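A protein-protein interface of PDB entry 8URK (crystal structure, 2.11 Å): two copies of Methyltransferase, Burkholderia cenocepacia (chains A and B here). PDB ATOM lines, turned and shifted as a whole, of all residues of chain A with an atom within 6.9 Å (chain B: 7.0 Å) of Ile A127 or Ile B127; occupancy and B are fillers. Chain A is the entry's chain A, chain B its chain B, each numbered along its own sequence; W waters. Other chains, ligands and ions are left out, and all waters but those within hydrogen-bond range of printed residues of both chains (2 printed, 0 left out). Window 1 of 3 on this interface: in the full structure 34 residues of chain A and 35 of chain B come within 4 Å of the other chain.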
ATOM      1  N   GLU A 125      36.684  28.002 -26.343  1.00  0.00           N
ATOM      2  CA  GLU A 125      35.763  28.993 -25.855  1.00  0.00           C
ATOM      3  C   GLU A 125      34.520  28.157 -25.598  1.00  0.00           C
ATOM      4  O   GLU A 125      33.978  27.552 -26.494  1.00  0.00           O
ATOM      5  CB  GLU A 125      35.462  30.133 -26.800  1.00  0.00           C
ATOM      6  CG  GLU A 125      34.066  30.693 -26.548  1.00  0.00           C
ATOM      7  CD  GLU A 125      33.736  31.933 -27.349  1.00  0.00           C
ATOM      8  OE1 GLU A 125      33.152  31.798 -28.431  1.00  0.00           O
ATOM      9  OE2 GLU A 125      34.048  33.040 -26.892  1.00  0.00           O
ATOM     10  N   ILE A 126      34.111  28.111 -24.358  1.00  0.00           N
ATOM     11  CA  ILE A 126      32.930  27.347 -23.992  1.00  0.00           C
ATOM     12  C   ILE A 126      31.781  28.318 -23.795  1.00  0.00           C
ATOM     13  O   ILE A 126      31.936  29.364 -23.154  1.00  0.00           O
ATOM     14  CB  ILE A 126      33.162  26.493 -22.735  1.00  0.00           C
ATOM     15  CG1 ILE A 126      34.073  25.297 -23.055  1.00  0.00           C
ATOM     16  CG2 ILE A 126      31.852  25.999 -22.209  1.00  0.00           C
ATOM     17  CD1 ILE A 126      35.451  25.460 -22.531  1.00  0.00           C
ATOM     18  N   ILE A 127      30.673  27.977 -24.384  1.00  0.00           N
ATOM     19  CA  ILE A 127      29.500  28.794 -24.288  1.00  0.00           C
ATOM     20  C   ILE A 127      28.571  28.142 -23.310  1.00  0.00           C
ATOM     21  O   ILE A 127      28.110  27.056 -23.532  1.00  0.00           O
ATOM     22  CB  ILE A 127      28.821  28.938 -25.680  1.00  0.00           C
ATOM     23  CG1 ILE A 127      29.797  29.515 -26.708  1.00  0.00           C
ATOM     24  CG2 ILE A 127      27.550  29.768 -25.582  1.00  0.00           C
ATOM     25  CD1 ILE A 127      30.297  30.902 -26.398  1.00  0.00           C
ATOM     26  N   TRP A 128      28.308  28.807 -22.220  1.00  0.00           N
ATOM     27  CA  TRP A 128      27.337  28.293 -21.294  1.00  0.00           C
ATOM     28  C   TRP A 128      25.966  28.802 -21.683  1.00  0.00           C
ATOM     29  O   TRP A 128      25.664  29.973 -21.536  1.00  0.00           O
ATOM     30  CB  TRP A 128      27.651  28.635 -19.850  1.00  0.00           C
ATOM     31  CG  TRP A 128      26.599  28.218 -18.898  1.00  0.00           C
ATOM     32  CD1 TRP A 128      25.869  27.079 -18.942  1.00  0.00           C
ATOM     33  CD2 TRP A 128      26.138  28.944 -17.762  1.00  0.00           C
ATOM     34  NE1 TRP A 128      24.991  27.038 -17.902  1.00  0.00           N
ATOM     35  CE2 TRP A 128      25.132  28.176 -17.160  1.00  0.00           C
ATOM     36  CE3 TRP A 128      26.480  30.168 -17.191  1.00  0.00           C
ATOM     37  CZ2 TRP A 128      24.461  28.591 -16.023  1.00  0.00           C
ATOM     38  CZ3 TRP A 128      25.817  30.575 -16.059  1.00  0.00           C
ATOM     39  CH2 TRP A 128      24.821  29.791 -15.486  1.00  0.00           C
ATOM     40  N   ASP A 129      25.167  27.913 -22.199  1.00  0.00           N
ATOM     41  CA  ASP A 129      23.826  28.241 -22.554  1.00  0.00           C
ATOM     42  C   ASP A 129      23.034  28.080 -21.284  1.00  0.00           C
ATOM     43  O   ASP A 129      22.899  26.990 -20.769  1.00  0.00           O
ATOM     44  CB  ASP A 129      23.332  27.355 -23.674  1.00  0.00           C
ATOM     45  CG  ASP A 129      21.832  27.396 -23.843  1.00  0.00           C
ATOM     46  OD1 ASP A 129      21.189  28.335 -23.355  1.00  0.00           O
ATOM     47  OD2 ASP A 129      21.298  26.475 -24.474  1.00  0.00           O
ATOM     48  N   ARG A 130      22.475  29.160 -20.817  1.00  0.00           N
ATOM     49  CA  ARG A 130      21.799  29.148 -19.553  1.00  0.00           C
ATOM     50  C   ARG A 130      20.347  28.794 -19.635  1.00  0.00           C
ATOM     51  O   ARG A 130      19.702  28.700 -18.614  1.00  0.00           O
ATOM     52  CB  ARG A 130      22.002  30.510 -18.926  1.00  0.00           C
ATOM     53  CG  ARG A 130      23.445  30.854 -18.631  1.00  0.00           C
ATOM     54  CD  ARG A 130      23.757  32.283 -19.025  1.00  0.00           C
ATOM     55  NE  ARG A 130      22.784  33.212 -18.474  1.00  0.00           N
ATOM     56  CZ  ARG A 130      22.562  34.431 -18.945  1.00  0.00           C
ATOM     57  NH1 ARG A 130      23.240  34.879 -19.984  1.00  0.00           N
ATOM     58  NH2 ARG A 130      21.658  35.202 -18.376  1.00  0.00           N
ATOM     59  N   VAL A 145      21.253  34.913 -23.174  1.00  0.00           N
ATOM     60  CA  VAL A 145      21.002  33.570 -22.663  1.00  0.00           C
ATOM     61  C   VAL A 145      22.294  32.771 -22.568  1.00  0.00           C
ATOM     62  O   VAL A 145      22.275  31.602 -22.161  1.00  0.00           O
ATOM     63  CB  VAL A 145      19.965  32.829 -23.529  1.00  0.00           C
ATOM     64  CG1 VAL A 145      20.617  32.314 -24.800  1.00  0.00           C
ATOM     65  CG2 VAL A 145      19.359  31.680 -22.758  1.00  0.00           C
ATOM     66  N   HIS A 146      23.431  33.381 -22.917  1.00  0.00           N
ATOM     67  CA  HIS A 146      24.711  32.699 -22.774  1.00  0.00           C
ATOM     68  C   HIS A 146      25.721  33.553 -22.018  1.00  0.00           C
ATOM     69  O   HIS A 146      25.703  34.788 -22.079  1.00  0.00           O
ATOM     70  CB  HIS A 146      25.293  32.273 -24.155  1.00  0.00           C
ATOM     71  CG  HIS A 146      25.978  33.366 -24.916  1.00  0.00           C
ATOM     72  ND1 HIS A 146      25.291  34.282 -25.675  1.00  0.00           N
ATOM     73  CD2 HIS A 146      27.290  33.660 -25.073  1.00  0.00           C
ATOM     74  CE1 HIS A 146      26.150  35.111 -26.247  1.00  0.00           C
ATOM     75  NE2 HIS A 146      27.369  34.750 -25.905  1.00  0.00           N
ATOM     76  N   ASP A 147      26.582  32.872 -21.270  1.00  0.00           N
ATOM     77  CA  ASP A 147      27.800  33.451 -20.724  1.00  0.00           C
ATOM     78  C   ASP A 147      28.972  32.871 -21.497  1.00  0.00           C
ATOM     79  O   ASP A 147      28.870  31.780 -22.064  1.00  0.00           O
ATOM     80  CB  ASP A 147      27.966  33.142 -19.233  1.00  0.00           C
ATOM     81  CG  ASP A 147      26.970  33.894 -18.358  1.00  0.00           C
ATOM     82  OD1 ASP A 147      26.218  34.732 -18.892  1.00  0.00           O
ATOM     83  OD2 ASP A 147      26.940  33.646 -17.133  1.00  0.00           O
ATOM     84  N   ASN A 148      30.080  33.600 -21.527  1.00  0.00           N
ATOM     85  CA  ASN A 148      31.272  33.171 -22.249  1.00  0.00           C
ATOM     86  C   ASN A 148      32.294  32.601 -21.267  1.00  0.00           C
ATOM     87  O   ASN A 148      32.551  33.196 -20.214  1.00  0.00           O
ATOM     88  CB  ASN A 148      31.880  34.334 -23.036  1.00  0.00           C
ATOM     89  CG  ASN A 148      31.000  34.776 -24.212  1.00  0.00           C
ATOM     90  OD1 ASN A 148      29.971  35.425 -24.016  1.00  0.00           O
ATOM     91  ND2 ASN A 148      31.423  34.454 -25.435  1.00  0.00           N
ATOM     92  N   ILE A 149      32.862  31.445 -21.603  1.00  0.00           N
ATOM     93  CA  ILE A 149      33.919  30.828 -20.810  1.00  0.00           C
ATOM     94  C   ILE A 149      35.135  30.645 -21.700  1.00  0.00           C
ATOM     95  O   ILE A 149      35.051  29.997 -22.749  1.00  0.00           O
ATOM     96  CB  ILE A 149      33.497  29.477 -20.221  1.00  0.00           C
ATOM     97  CG1 ILE A 149      32.170  29.600 -19.488  1.00  0.00           C
ATOM     98  CG2 ILE A 149      34.594  28.953 -19.304  1.00  0.00           C
ATOM     99  CD1 ILE A 149      31.507  28.255 -19.260  1.00  0.00           C
ATOM    100  N   LYS A 195      31.320  19.076 -25.899  1.00  0.00           N
ATOM    101  CA  LYS A 195      31.387  20.118 -26.921  1.00  0.00           C
ATOM    102  C   LYS A 195      31.646  21.498 -26.291  1.00  0.00           C
ATOM    103  O   LYS A 195      31.816  21.573 -25.096  1.00  0.00           O
ATOM    104  CB  LYS A 195      30.164  20.095 -27.837  1.00  0.00           C
ATOM    105  CG  LYS A 195      29.699  18.741 -28.313  1.00  0.00           C
ATOM    106  CD  LYS A 195      28.310  18.865 -28.903  1.00  0.00           C
ATOM    107  CE  LYS A 195      27.858  17.590 -29.572  1.00  0.00           C
ATOM    108  NZ  LYS A 195      27.249  16.686 -28.571  1.00  0.00           N
ATOM    109  N   ASP A 196      31.721  22.554 -27.095  1.00  0.00           N
ATOM    110  CA  ASP A 196      31.996  23.902 -26.596  1.00  0.00           C
ATOM    111  C   ASP A 196      30.735  24.704 -26.294  1.00  0.00           C
ATOM    112  O   ASP A 196      30.805  25.886 -26.079  1.00  0.00           O
ATOM    113  CB  ASP A 196      32.963  24.679 -27.504  1.00  0.00           C
ATOM    114  CG  ASP A 196      32.558  24.703 -28.920  1.00  0.00           C
ATOM    115  OD1 ASP A 196      31.384  24.458 -29.232  1.00  0.00           O
ATOM    116  OD2 ASP A 196      33.441  24.993 -29.727  1.00  0.00           O
ATOM    117  N   VAL A 197      29.591  24.069 -26.321  1.00  0.00           N
ATOM    118  CA  VAL A 197      28.372  24.727 -25.886  1.00  0.00           C
ATOM    119  C   VAL A 197      27.770  23.850 -24.796  1.00  0.00           C
ATOM    120  O   VAL A 197      27.410  22.724 -25.043  1.00  0.00           O
ATOM    121  CB  VAL A 197      27.358  25.037 -27.020  1.00  0.00           C
ATOM    122  CG1 VAL A 197      26.191  25.827 -26.462  1.00  0.00           C
ATOM    123  CG2 VAL A 197      28.023  25.771 -28.167  1.00  0.00           C
ATOM    124  N   TRP A 198      27.685  24.373 -23.594  1.00  0.00           N
ATOM    125  CA  TRP A 198      27.113  23.638 -22.477  1.00  0.00           C
ATOM    126  C   TRP A 198      25.730  24.133 -22.097  1.00  0.00           C
ATOM    127  O   TRP A 198      25.575  25.211 -21.555  1.00  0.00           O
ATOM    128  CB  TRP A 198      28.054  23.640 -21.254  1.00  0.00           C
ATOM    129  CG  TRP A 198      29.441  23.153 -21.502  1.00  0.00           C
ATOM    130  CD1 TRP A 198      29.906  22.525 -22.611  1.00  0.00           C
ATOM    131  CD2 TRP A 198      30.551  23.251 -20.606  1.00  0.00           C
ATOM    132  NE1 TRP A 198      31.234  22.235 -22.469  1.00  0.00           N
ATOM    133  CE2 TRP A 198      31.654  22.670 -21.244  1.00  0.00           C
ATOM    134  CE3 TRP A 198      30.716  23.778 -19.329  1.00  0.00           C
ATOM    135  CZ2 TRP A 198      32.911  22.600 -20.647  1.00  0.00           C
ATOM    136  CZ3 TRP A 198      31.961  23.705 -18.739  1.00  0.00           C
ATOM    137  CH2 TRP A 198      33.040  23.124 -19.398  1.00  0.00           C
ATOM    138  N   SER A 199      24.733  23.332 -22.387  1.00  0.00           N
ATOM    139  CA  SER A 199      23.368  23.674 -22.066  1.00  0.00           C
ATOM    140  C   SER A 199      23.028  23.194 -20.674  1.00  0.00           C
ATOM    141  O   SER A 199      22.772  22.023 -20.469  1.00  0.00           O
ATOM    142  CB  SER A 199      22.410  23.081 -23.085  1.00  0.00           C
ATOM    143  OG  SER A 199      22.308  23.889 -24.231  1.00  0.00           O
ATOM    144  N   GLU B 125      25.927  39.438 -29.269  1.00  0.00           N
ATOM    145  CA  GLU B 125      26.864  38.428 -29.715  1.00  0.00           C
ATOM    146  C   GLU B 125      25.955  37.229 -29.788  1.00  0.00           C
ATOM    147  O   GLU B 125      25.443  36.766 -28.788  1.00  0.00           O
ATOM    148  CB  GLU B 125      28.034  38.188 -28.796  1.00  0.00           C
ATOM    149  CG  GLU B 125      29.058  37.211 -29.357  1.00  0.00           C
ATOM    150  CD  GLU B 125      29.658  36.257 -28.330  1.00  0.00           C
ATOM    151  OE1 GLU B 125      29.240  36.253 -27.164  1.00  0.00           O
ATOM    152  OE2 GLU B 125      30.566  35.503 -28.702  1.00  0.00           O
ATOM    153  N   ILE B 126      25.706  36.767 -30.990  1.00  0.00           N
ATOM    154  CA  ILE B 126      24.816  35.643 -31.216  1.00  0.00           C
ATOM    155  C   ILE B 126      25.661  34.392 -31.385  1.00  0.00           C
ATOM    156  O   ILE B 126      26.603  34.374 -32.186  1.00  0.00           O
ATOM    157  CB  ILE B 126      23.909  35.880 -32.435  1.00  0.00           C
ATOM    158  CG1 ILE B 126      22.941  37.035 -32.162  1.00  0.00           C
ATOM    159  CG2 ILE B 126      23.085  34.655 -32.720  1.00  0.00           C
ATOM    160  CD1 ILE B 126      22.897  38.032 -33.252  1.00  0.00           C
ATOM    161  N   ILE B 127      25.316  33.348 -30.644  1.00  0.00           N
ATOM    162  CA  ILE B 127      25.991  32.063 -30.741  1.00  0.00           C
ATOM    163  C   ILE B 127      25.153  31.175 -31.648  1.00  0.00           C
ATOM    164  O   ILE B 127      24.006  30.848 -31.326  1.00  0.00           O
ATOM    165  CB  ILE B 127      26.195  31.426 -29.358  1.00  0.00           C
ATOM    166  CG1 ILE B 127      26.957  32.394 -28.454  1.00  0.00           C
ATOM    167  CG2 ILE B 127      26.965  30.103 -29.481  1.00  0.00           C
ATOM    168  CD1 ILE B 127      28.429  32.533 -28.843  1.00  0.00           C
ATOM    169  N   TRP B 128      25.726  30.740 -32.736  1.00  0.00           N
ATOM    170  CA  TRP B 128      25.051  29.757 -33.548  1.00  0.00           C
ATOM    171  C   TRP B 128      25.451  28.382 -33.040  1.00  0.00           C
ATOM    172  O   TRP B 128      26.575  27.962 -33.213  1.00  0.00           O
ATOM    173  CB  TRP B 128      25.344  29.887 -35.016  1.00  0.00           C
ATOM    174  CG  TRP B 128      24.725  28.804 -35.832  1.00  0.00           C
ATOM    175  CD1 TRP B 128      23.558  28.160 -35.577  1.00  0.00           C
ATOM    176  CD2 TRP B 128      25.250  28.219 -37.025  1.00  0.00           C
ATOM    177  NE1 TRP B 128      23.316  27.222 -36.534  1.00  0.00           N
ATOM    178  CE2 TRP B 128      24.340  27.233 -37.437  1.00  0.00           C
ATOM    179  CE3 TRP B 128      26.400  28.432 -37.784  1.00  0.00           C
ATOM    180  CZ2 TRP B 128      24.541  26.465 -38.575  1.00  0.00           C
ATOM    181  CZ3 TRP B 128      26.597  27.670 -38.911  1.00  0.00           C
ATOM    182  CH2 TRP B 128      25.670  26.701 -39.298  1.00  0.00           C
ATOM    183  N   ASP B 129      24.538  27.729 -32.382  1.00  0.00           N
ATOM    184  CA  ASP B 129      24.740  26.378 -31.944  1.00  0.00           C
ATOM    185  C   ASP B 129      24.427  25.497 -33.137  1.00  0.00           C
ATOM    186  O   ASP B 129      23.294  25.344 -33.521  1.00  0.00           O
ATOM    187  CB  ASP B 129      23.848  26.073 -30.770  1.00  0.00           C
ATOM    188  CG  ASP B 129      23.888  24.615 -30.345  1.00  0.00           C
ATOM    189  OD1 ASP B 129      24.646  23.816 -30.913  1.00  0.00           O
ATOM    190  OD2 ASP B 129      23.142  24.275 -29.414  1.00  0.00           O
ATOM    191  N   ARG B 130      25.451  24.909 -33.692  1.00  0.00           N
ATOM    192  CA  ARG B 130      25.320  24.093 -34.884  1.00  0.00           C
ATOM    193  C   ARG B 130      24.764  22.715 -34.625  1.00  0.00           C
ATOM    194  O   ARG B 130      24.424  22.032 -35.564  1.00  0.00           O
ATOM    195  CB  ARG B 130      26.684  24.051 -35.549  1.00  0.00           C
ATOM    196  CG  ARG B 130      27.119  25.351 -36.194  1.00  0.00           C
ATOM    197  CD  ARG B 130      28.619  25.541 -36.081  1.00  0.00           C
ATOM    198  NE  ARG B 130      29.355  24.301 -36.295  1.00  0.00           N
ATOM    199  CZ  ARG B 130      30.586  24.082 -35.860  1.00  0.00           C
ATOM    200  NH1 ARG B 130      31.229  25.010 -35.186  1.00  0.00           N
ATOM    201  NH2 ARG B 130      31.175  22.929 -36.099  1.00  0.00           N
ATOM    202  N   VAL B 145      30.938  23.027 -31.566  1.00  0.00           N
ATOM    203  CA  VAL B 145      29.542  22.978 -31.991  1.00  0.00           C
ATOM    204  C   VAL B 145      28.944  24.389 -32.109  1.00  0.00           C
ATOM    205  O   VAL B 145      27.743  24.530 -32.197  1.00  0.00           O
ATOM    206  CB  VAL B 145      28.699  22.113 -31.061  1.00  0.00           C
ATOM    207  CG1 VAL B 145      28.489  22.793 -29.722  1.00  0.00           C
ATOM    208  CG2 VAL B 145      27.398  21.688 -31.712  1.00  0.00           C
ATOM    209  N   HIS B 146      29.775  25.416 -32.116  1.00  0.00           N
ATOM    210  CA  HIS B 146      29.307  26.792 -32.284  1.00  0.00           C
ATOM    211  C   HIS B 146      30.169  27.714 -33.117  1.00  0.00           C
ATOM    212  O   HIS B 146      31.372  27.628 -33.074  1.00  0.00           O
ATOM    213  CB  HIS B 146      29.055  27.448 -30.910  1.00  0.00           C
ATOM    214  CG  HIS B 146      30.245  28.109 -30.298  1.00  0.00           C
ATOM    215  ND1 HIS B 146      31.304  27.404 -29.776  1.00  0.00           N
ATOM    216  CD2 HIS B 146      30.526  29.416 -30.088  1.00  0.00           C
ATOM    217  CE1 HIS B 146      32.196  28.245 -29.293  1.00  0.00           C
ATOM    218  NE2 HIS B 146      31.745  29.473 -29.464  1.00  0.00           N
ATOM    219  N   ASP B 147      29.556  28.560 -33.913  1.00  0.00           N
ATOM    220  CA  ASP B 147      30.263  29.589 -34.646  1.00  0.00           C
ATOM    221  C   ASP B 147      29.817  30.883 -33.959  1.00  0.00           C
ATOM    222  O   ASP B 147      28.819  30.896 -33.273  1.00  0.00           O
ATOM    223  CB  ASP B 147      29.924  29.668 -36.123  1.00  0.00           C
ATOM    224  CG  ASP B 147      30.320  28.432 -36.894  1.00  0.00           C
ATOM    225  OD1 ASP B 147      31.047  27.583 -36.355  1.00  0.00           O
ATOM    226  OD2 ASP B 147      29.899  28.318 -38.055  1.00  0.00           O
ATOM    227  N   ASN B 148      30.550  31.955 -34.140  1.00  0.00           N
ATOM    228  CA  ASN B 148      30.236  33.224 -33.515  1.00  0.00           C
ATOM    229  C   ASN B 148      29.707  34.260 -34.485  1.00  0.00           C
ATOM    230  O   ASN B 148      30.178  34.377 -35.596  1.00  0.00           O
ATOM    231  CB  ASN B 148      31.460  33.809 -32.816  1.00  0.00           C
ATOM    232  CG  ASN B 148      32.020  32.899 -31.734  1.00  0.00           C
ATOM    233  OD1 ASN B 148      32.596  31.860 -32.023  1.00  0.00           O
ATOM    234  ND2 ASN B 148      31.866  33.300 -30.489  1.00  0.00           N
ATOM    235  N   ILE B 149      28.745  35.023 -34.037  1.00  0.00           N
ATOM    236  CA  ILE B 149      28.208  36.088 -34.866  1.00  0.00           C
ATOM    237  C   ILE B 149      28.164  37.405 -34.107  1.00  0.00           C
ATOM    238  O   ILE B 149      27.595  37.478 -33.036  1.00  0.00           O
ATOM    239  CB  ILE B 149      26.819  35.767 -35.408  1.00  0.00           C
ATOM    240  CG1 ILE B 149      26.786  34.394 -36.082  1.00  0.00           C
ATOM    241  CG2 ILE B 149      26.376  36.856 -36.375  1.00  0.00           C
ATOM    242  CD1 ILE B 149      25.401  33.814 -36.178  1.00  0.00           C
ATOM    243  N   LYS B 195      16.548  35.025 -28.782  1.00  0.00           N
ATOM    244  CA  LYS B 195      17.694  35.048 -27.874  1.00  0.00           C
ATOM    245  C   LYS B 195      19.010  35.111 -28.636  1.00  0.00           C
ATOM    246  O   LYS B 195      19.006  35.106 -29.869  1.00  0.00           O
ATOM    247  CB  LYS B 195      17.666  33.838 -26.942  1.00  0.00           C
ATOM    248  CG  LYS B 195      16.286  33.533 -26.407  1.00  0.00           C
ATOM    249  CD  LYS B 195      16.325  32.882 -25.023  1.00  0.00           C
ATOM    250  CE  LYS B 195      15.380  31.730 -24.980  1.00  0.00           C
ATOM    251  NZ  LYS B 195      14.044  32.220 -25.354  1.00  0.00           N
ATOM    252  N   ASP B 196      20.140  35.174 -27.927  1.00  0.00           N
ATOM    253  CA  ASP B 196      21.438  35.249 -28.587  1.00  0.00           C
ATOM    254  C   ASP B 196      22.157  33.908 -28.608  1.00  0.00           C
ATOM    255  O   ASP B 196      23.383  33.870 -28.753  1.00  0.00           O
ATOM    256  CB  ASP B 196      22.333  36.309 -27.943  1.00  0.00           C
ATOM    257  CG  ASP B 196      22.714  35.961 -26.541  1.00  0.00           C
ATOM    258  OD1 ASP B 196      22.448  34.816 -26.126  1.00  0.00           O
ATOM    259  OD2 ASP B 196      23.304  36.823 -25.860  1.00  0.00           O
ATOM    260  N   VAL B 197      21.425  32.815 -28.437  1.00  0.00           N
ATOM    261  CA  VAL B 197      21.899  31.484 -28.789  1.00  0.00           C
ATOM    262  C   VAL B 197      20.880  30.917 -29.752  1.00  0.00           C
ATOM    263  O   VAL B 197      19.687  30.858 -29.430  1.00  0.00           O
ATOM    264  CB  VAL B 197      22.057  30.555 -27.575  1.00  0.00           C
ATOM    265  CG1 VAL B 197      22.587  29.217 -28.054  1.00  0.00           C
ATOM    266  CG2 VAL B 197      22.993  31.152 -26.520  1.00  0.00           C
ATOM    267  N   TRP B 198      21.336  30.532 -30.920  1.00  0.00           N
ATOM    268  CA  TRP B 198      20.469  29.970 -31.925  1.00  0.00           C
ATOM    269  C   TRP B 198      20.809  28.527 -32.208  1.00  0.00           C
ATOM    270  O   TRP B 198      21.814  28.236 -32.833  1.00  0.00           O
ATOM    271  CB  TRP B 198      20.519  30.804 -33.189  1.00  0.00           C
ATOM    272  CG  TRP B 198      20.105  32.215 -33.095  1.00  0.00           C
ATOM    273  CD1 TRP B 198      19.495  32.831 -32.056  1.00  0.00           C
ATOM    274  CD2 TRP B 198      20.259  33.201 -34.114  1.00  0.00           C
ATOM    275  NE1 TRP B 198      19.264  34.144 -32.358  1.00  0.00           N
ATOM    276  CE2 TRP B 198      19.726  34.399 -33.617  1.00  0.00           C
ATOM    277  CE3 TRP B 198      20.798  33.187 -35.398  1.00  0.00           C
ATOM    278  CZ2 TRP B 198      19.714  35.572 -34.359  1.00  0.00           C
ATOM    279  CZ3 TRP B 198      20.785  34.348 -36.129  1.00  0.00           C
ATOM    280  CH2 TRP B 198      20.247  35.526 -35.608  1.00  0.00           C
ATOM    281  N   SER B 199      19.977  27.639 -31.712  1.00  0.00           N
ATOM    282  CA  SER B 199      20.178  26.234 -31.912  1.00  0.00           C
ATOM    283  C   SER B 199      19.538  25.779 -33.213  1.00  0.00           C
ATOM    284  O   SER B 199      18.379  25.445 -33.245  1.00  0.00           O
ATOM    285  CB  SER B 199      19.664  25.437 -30.716  1.00  0.00           C
ATOM    286  OG  SER B 199      20.427  25.700 -29.562  1.00  0.00           O
ATOM    287  N   VAL B 200      20.317  25.782 -34.267  1.00  0.00           N
ATOM    288  CA  VAL B 200      19.843  25.365 -35.581  1.00  0.00           C
ATOM    289  C   VAL B 200      20.910  24.461 -36.176  1.00  0.00           C
ATOM    290  O   VAL B 200      22.032  24.855 -36.347  1.00  0.00           O
ATOM    291  CB  VAL B 200      19.510  26.556 -36.509  1.00  0.00           C
ATOM    292  CG1 VAL B 200      19.115  26.066 -37.890  1.00  0.00           C
ATOM    293  CG2 VAL B 200      18.444  27.440 -35.896  1.00  0.00           C
HETATM  294  O   HOH W   1      33.575  26.125 -32.121  1.00  0.00           O
HETATM  295  O   HOH W   2      24.400  37.063 -23.272  1.00  0.00           O
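The guanidinium group of Arg A130 lies within hydrogen-bond range of the backbone carbonyl oxygen of His A146, 3.2 Å away.
ND2 of Asn B148 sits at hydrogen-bond distance from OE2 of Glu B125 (3.1 Å).
N of Ile B127 lies within hydrogen-bond range of O of Asp B196 (2.8 Å).
N of Trp B198 lies within hydrogen-bond range of O of Ile B127.
O of His B146 lies within hydrogen-bond range of NH1 of Arg B130 (3.4 Å).
O of Lys B195 sits at hydrogen-bond distance from NE1 of Trp B198, 2.7 Å away.
Glu A125 touches Asn B148, and with the chains exchanged Asn A148 touches Glu B125.
Ile A127 touches its own counterpart, Ile B127.
Ile A127 touches His B146, and with the chains exchanged His A146 touches Ile B127.
Val A145 touches Lys B195, and with the chains exchanged Lys A195 touches Val B145.
16 positions are printed for both chains.
Of the 17 pairs that touch across the chains among the printed residues, 17 have their exchanged pair printed and touching as well.
Among the printed residues, pairs that only touch across the chains: Ile A127 with Ile B127 (3.5 Å), Ile A127 with His B146 (3.4 Å), Val A145 with Lys B195 (3.9 Å), Val A145 with Val B197 (3.2 Å), His A146 with Ile B127 (3.5 Å), His A146 with Val B197 (3.5 Å), Lys A195 with Val B145 (3.7 Å), Val A197 with Val B145 (3.4 Å) and Val A197 with His B146 (3.4 Å).
Water W1 lies within hydrogen-bond range of OD2 of Asp A196 and O of His B146.
Water W2 lies within hydrogen-bond range of the side-chain carboxylate of Asp B196 and the backbone carbonyl oxygen of His A146.
OE1 of Glu A125 lies within hydrogen-bond range of NE2 of His B146 (2.9 Å).
The side-chain amide nitrogen (ND2) of Asn B148 lies within hydrogen-bond range of the side-chain carboxylate (OE1) of Glu A125 (2.9 Å).
The backbone NH (N) of Val A145 is in hydrogen-bond range of the side-chain carboxylate (OD1) of Asp B196, at 3.2 Å.
The side-chain carboxylate (OE1) of Glu B125 lies within hydrogen-bond range of a ring nitrogen (NE2) of His A146.
A ring nitrogen (ND1) of His A146 sits at hydrogen-bond distance from the side-chain carboxylate (OD1) of Asp B196, 2.9 Å away.
ND2 of Asn A148 sits at hydrogen-bond distance from OE1 of Glu B125, at 3.3 Å.
The side-chain carboxylate (OD1) of Asp A196 sits at hydrogen-bond distance from the backbone NH (N) of Val B145 (2.8 Å).
ND1 of His B146 sits at hydrogen-bond distance from OD1 of Asp A196, 3.0 Å away.
Ile A127 touches just these residues of chain B: Ile B127 (3.5 Å) and His B146 (3.4 Å).
Printed residues of chain A within 4 Å of Ile B127: Ile A127 and His A146.
Of the printed residues of chain A, His B146 touches Glu A125 (2.9 Å), Ile A127 (3.4 Å), Asp A196 (3.0 Å) and Val A197 (3.4 Å).
Printed residues of chain B within 4 Å of Glu A125: His B146 and Asn B148.
Of the printed residues of chain B, Val A197 touches Val B145 and His B146.
Of the printed residues of chain B, Asn A148 touches Glu B125.
Printed residues of chain B within 4 Å of Val A145: Lys B195 (3.9 Å), Asp B196 (3.2 Å) and Val B197 (3.2 Å).
Ile B126 touches none of the printed residues of chain A.
The nearest residue of chain B that does not touch Ile A127 is Val B197 (4.9 Å).
Printed residues of chain A that touch a printed residue of chain B: Glu A125, Ile A127, Val A145, His A146, Asn A148, Lys A195, Asp A196 and Val A197.
Hydrophobic or aromatic side chains of chain A within 4 Å of the printed part of chain B: Ile A127, Val A145, His A146 and Val A197.
Printed residues of chain B that touch a printed residue of chain A: Glu B125, Ile B127, Val B145, His B146, Asn B148, Lys B195, Asp B196 and Val B197.
Along chain B the printed residues that touch a printed residue of chain A span positions 125 to 197.
Among the printed residues, 17 pairs touch across the chains.
Among the printed residues, no Asp or Glu carboxylate lies within 4 Å of a Lys or Arg side-chain nitrogen of the other chain.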
